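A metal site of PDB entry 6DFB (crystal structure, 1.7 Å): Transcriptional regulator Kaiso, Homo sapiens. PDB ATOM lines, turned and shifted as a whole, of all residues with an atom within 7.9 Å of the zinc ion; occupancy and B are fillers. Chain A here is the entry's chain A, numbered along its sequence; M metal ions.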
ATOM      1  N   PRO A  53      -1.202  -0.815  25.203  1.00  0.00           N
ATOM      2  CA  PRO A  53      -1.113   0.307  26.135  1.00  0.00           C
ATOM      3  C   PRO A  53      -0.290  -0.012  27.371  1.00  0.00           C
ATOM      4  O   PRO A  53      -0.476  -1.076  27.953  1.00  0.00           O
ATOM      5  CB  PRO A  53      -2.566   0.550  26.531  1.00  0.00           C
ATOM      6  CG  PRO A  53      -3.216  -0.773  26.386  1.00  0.00           C
ATOM      7  CD  PRO A  53      -2.528  -1.452  25.225  1.00  0.00           C
ATOM      8  N   CYS A  54       0.621   0.895  27.736  1.00  0.00           N
ATOM      9  CA  CYS A  54       1.362   0.777  29.000  1.00  0.00           C
ATOM     10  C   CYS A  54       0.351   0.745  30.129  1.00  0.00           C
ATOM     11  O   CYS A  54      -0.648   1.468  30.112  1.00  0.00           O
ATOM     12  CB  CYS A  54       2.329   1.951  29.167  1.00  0.00           C
ATOM     13  SG  CYS A  54       3.304   1.942  30.707  1.00  0.00           S
ATOM     14  N   ARG A  55       0.597  -0.082  31.127  1.00  0.00           N
ATOM     15  CA  ARG A  55      -0.343  -0.195  32.226  1.00  0.00           C
ATOM     16  C   ARG A  55       0.055   0.708  33.395  1.00  0.00           C
ATOM     17  O   ARG A  55      -0.582   0.711  34.452  1.00  0.00           O
ATOM     18  CB  ARG A  55      -0.479  -1.653  32.658  1.00  0.00           C
ATOM     19  CG  ARG A  55      -1.596  -2.341  31.886  1.00  0.00           C
ATOM     20  CD  ARG A  55      -1.256  -3.749  31.434  1.00  0.00           C
ATOM     21  NE  ARG A  55      -0.006  -3.844  30.681  1.00  0.00           N
ATOM     22  CZ  ARG A  55       0.453  -4.980  30.178  1.00  0.00           C
ATOM     23  NH1 ARG A  55      -0.249  -6.104  30.338  1.00  0.00           N
ATOM     24  NH2 ARG A  55       1.603  -5.020  29.520  1.00  0.00           N
ATOM     25  N   TYR A  56       1.094   1.519  33.180  1.00  0.00           N
ATOM     26  CA  TYR A  56       1.609   2.431  34.206  1.00  0.00           C
ATOM     27  C   TYR A  56       1.540   3.885  33.779  1.00  0.00           C
ATOM     28  O   TYR A  56       1.625   4.797  34.620  1.00  0.00           O
ATOM     29  CB  TYR A  56       3.048   2.072  34.564  1.00  0.00           C
ATOM     30  CG  TYR A  56       3.242   0.648  34.986  1.00  0.00           C
ATOM     31  CD1 TYR A  56       3.174   0.284  36.326  1.00  0.00           C
ATOM     32  CD2 TYR A  56       3.515  -0.342  34.056  1.00  0.00           C
ATOM     33  CE1 TYR A  56       3.375  -1.028  36.716  1.00  0.00           C
ATOM     34  CE2 TYR A  56       3.703  -1.651  34.440  1.00  0.00           C
ATOM     35  CZ  TYR A  56       3.633  -1.993  35.781  1.00  0.00           C
ATOM     36  OH  TYR A  56       3.818  -3.301  36.156  1.00  0.00           O
ATOM     37  N   CYS A  57       1.401   4.122  32.474  1.00  0.00           N
ATOM     38  CA  CYS A  57       1.228   5.474  31.945  1.00  0.00           C
ATOM     39  C   CYS A  57       0.388   5.434  30.673  1.00  0.00           C
ATOM     40  O   CYS A  57      -0.148   4.389  30.318  1.00  0.00           O
ATOM     41  CB  CYS A  57       2.583   6.150  31.677  1.00  0.00           C
ATOM     42  SG  CYS A  57       3.421   5.626  30.171  1.00  0.00           S
ATOM     43  N   GLU A  58       0.268   6.571  29.999  1.00  0.00           N
ATOM     44  CA  GLU A  58      -0.633   6.746  28.854  1.00  0.00           C
ATOM     45  C   GLU A  58      -0.100   6.229  27.522  1.00  0.00           C
ATOM     46  O   GLU A  58      -0.826   6.190  26.528  1.00  0.00           O
ATOM     47  CB  GLU A  58      -0.999   8.227  28.716  1.00  0.00           C
ATOM     48  CG  GLU A  58       0.146   9.143  28.236  1.00  0.00           C
ATOM     49  CD  GLU A  58       1.310   9.245  29.232  1.00  0.00           C
ATOM     50  OE1 GLU A  58       2.462   9.376  28.782  1.00  0.00           O
ATOM     51  OE2 GLU A  58       1.070   9.182  30.454  1.00  0.00           O
ATOM     52  N   LYS A  59       1.172   5.853  27.483  1.00  0.00           N
ATOM     53  CA  LYS A  59       1.811   5.477  26.221  1.00  0.00           C
ATOM     54  C   LYS A  59       1.241   4.203  25.604  1.00  0.00           C
ATOM     55  O   LYS A  59       0.820   3.287  26.315  1.00  0.00           O
ATOM     56  CB  LYS A  59       3.327   5.331  26.426  1.00  0.00           C
ATOM     57  CG  LYS A  59       4.031   6.681  26.509  1.00  0.00           C
ATOM     58  CD  LYS A  59       5.540   6.544  26.577  1.00  0.00           C
ATOM     59  CE  LYS A  59       6.205   7.890  26.793  1.00  0.00           C
ATOM     60  NZ  LYS A  59       7.637   7.766  27.138  1.00  0.00           N
ATOM     61  N   VAL A  60       1.210   4.156  24.271  1.00  0.00           N
ATOM     62  CA  VAL A  60       0.665   3.012  23.562  1.00  0.00           C
ATOM     63  C   VAL A  60       1.677   2.543  22.516  1.00  0.00           C
ATOM     64  O   VAL A  60       2.278   3.368  21.829  1.00  0.00           O
ATOM     65  CB  VAL A  60      -0.673   3.354  22.873  1.00  0.00           C
ATOM     66  CG1 VAL A  60      -1.265   2.126  22.213  1.00  0.00           C
ATOM     67  CG2 VAL A  60      -1.656   3.928  23.889  1.00  0.00           C
ATOM     68  N   PHE A  61       1.846   1.230  22.403  1.00  0.00           N
ATOM     69  CA  PHE A  61       2.851   0.670  21.486  1.00  0.00           C
ATOM     70  C   PHE A  61       2.233  -0.212  20.404  1.00  0.00           C
ATOM     71  O   PHE A  61       1.156  -0.765  20.620  1.00  0.00           O
ATOM     72  CB  PHE A  61       3.891  -0.111  22.280  1.00  0.00           C
ATOM     73  CG  PHE A  61       4.603   0.722  23.302  1.00  0.00           C
ATOM     74  CD1 PHE A  61       5.802   1.340  22.986  1.00  0.00           C
ATOM     75  CD2 PHE A  61       4.037   0.944  24.552  1.00  0.00           C
ATOM     76  CE1 PHE A  61       6.449   2.132  23.914  1.00  0.00           C
ATOM     77  CE2 PHE A  61       4.679   1.749  25.483  1.00  0.00           C
ATOM     78  CZ  PHE A  61       5.882   2.332  25.154  1.00  0.00           C
ATOM     79  N   ARG A  67       6.094  -2.636  24.385  1.00  0.00           N
ATOM     80  CA  ARG A  67       5.443  -2.301  25.629  1.00  0.00           C
ATOM     81  C   ARG A  67       6.176  -2.956  26.817  1.00  0.00           C
ATOM     82  O   ARG A  67       6.393  -2.324  27.856  1.00  0.00           O
ATOM     83  CB  ARG A  67       3.988  -2.739  25.621  1.00  0.00           C
ATOM     84  CG  ARG A  67       3.364  -2.568  27.001  1.00  0.00           C
ATOM     85  CD  ARG A  67       1.905  -2.846  26.977  1.00  0.00           C
ATOM     86  NE  ARG A  67       1.611  -4.225  26.657  1.00  0.00           N
ATOM     87  CZ  ARG A  67       0.367  -4.699  26.585  1.00  0.00           C
ATOM     88  NH1 ARG A  67      -0.652  -3.891  26.805  1.00  0.00           N
ATOM     89  NH2 ARG A  67       0.152  -5.976  26.280  1.00  0.00           N
ATOM     90  N   HIS A  70       9.412  -1.207  27.794  1.00  0.00           N
ATOM     91  CA  HIS A  70       8.981   0.030  28.439  1.00  0.00           C
ATOM     92  C   HIS A  70       8.467  -0.183  29.862  1.00  0.00           C
ATOM     93  O   HIS A  70       8.790   0.578  30.755  1.00  0.00           O
ATOM     94  CB  HIS A  70       7.906   0.708  27.570  1.00  0.00           C
ATOM     95  CG  HIS A  70       7.247   1.885  28.216  1.00  0.00           C
ATOM     96  ND1 HIS A  70       7.837   3.123  28.265  1.00  0.00           N
ATOM     97  CD2 HIS A  70       6.054   2.000  28.840  1.00  0.00           C
ATOM     98  CE1 HIS A  70       7.027   3.966  28.887  1.00  0.00           C
ATOM     99  NE2 HIS A  70       5.938   3.304  29.234  1.00  0.00           N
ATOM    100  N   GLU A  71       7.647  -1.219  30.070  1.00  0.00           N
ATOM    101  CA  GLU A  71       7.088  -1.470  31.391  1.00  0.00           C
ATOM    102  C   GLU A  71       8.163  -1.913  32.374  1.00  0.00           C
ATOM    103  O   GLU A  71       8.064  -1.603  33.562  1.00  0.00           O
ATOM    104  CB  GLU A  71       5.983  -2.511  31.325  1.00  0.00           C
ATOM    105  CG  GLU A  71       4.761  -2.007  30.541  1.00  0.00           C
ATOM    106  CD  GLU A  71       3.549  -2.881  30.704  1.00  0.00           C
ATOM    107  OE1 GLU A  71       3.708  -4.107  30.876  1.00  0.00           O
ATOM    108  OE2 GLU A  71       2.424  -2.353  30.646  1.00  0.00           O
ATOM    109  N   HIS A  73      11.064  -0.678  32.448  1.00  0.00           N
ATOM    110  CA  HIS A  73      11.629   0.618  32.863  1.00  0.00           C
ATOM    111  C   HIS A  73      10.832   1.228  34.021  1.00  0.00           C
ATOM    112  O   HIS A  73      11.418   1.816  34.936  1.00  0.00           O
ATOM    113  CB  HIS A  73      11.664   1.607  31.694  1.00  0.00           C
ATOM    114  CG  HIS A  73      12.962   1.636  30.968  1.00  0.00           C
ATOM    115  ND1 HIS A  73      14.071   2.308  31.452  1.00  0.00           N
ATOM    116  CD2 HIS A  73      13.351   1.090  29.789  1.00  0.00           C
ATOM    117  CE1 HIS A  73      15.072   2.171  30.602  1.00  0.00           C
ATOM    118  NE2 HIS A  73      14.662   1.437  29.583  1.00  0.00           N
ATOM    119  N   HIS A  74       9.508   1.104  33.981  1.00  0.00           N
ATOM    120  CA  HIS A  74       8.682   1.589  35.073  1.00  0.00           C
ATOM    121  C   HIS A  74       9.024   0.903  36.403  1.00  0.00           C
ATOM    122  O   HIS A  74       9.103   1.571  37.433  1.00  0.00           O
ATOM    123  CB  HIS A  74       7.189   1.388  34.774  1.00  0.00           C
ATOM    124  CG  HIS A  74       6.565   2.467  33.931  1.00  0.00           C
ATOM    125  ND1 HIS A  74       6.348   3.741  34.417  1.00  0.00           N
ATOM    126  CD2 HIS A  74       6.072   2.448  32.673  1.00  0.00           C
ATOM    127  CE1 HIS A  74       5.757   4.470  33.477  1.00  0.00           C
ATOM    128  NE2 HIS A  74       5.582   3.704  32.417  1.00  0.00           N
HETATM  129 ZN    ZN M   1       4.503   3.723  30.639  1.00  0.00          ZN
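SG of Cys 54 lies close to N of Tyr 56 (3.3 Å).
The backbone carbonyl oxygen (O) of Lys 59 is in hydrogen-bond range of the backbone NH (N) of Cys 54.
N of Lys 59 lies close to SG of Cys 57 (3.5 Å).
The zinc ion is bound by a ring nitrogen (NE2) of His 70 (2.1 Å), a ring nitrogen (NE2) of His 74 (2.1 Å), the side-chain sulfur (SG) of Cys 54 (2.1 Å) and the side-chain sulfur (SG) of Cys 57 (2.2 Å).
Of the 14 residues printed, 4 come within 4 Å of the zinc ion.
The nearest printed residue that does not touch the zinc ion is Tyr 56 (4.3 Å).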
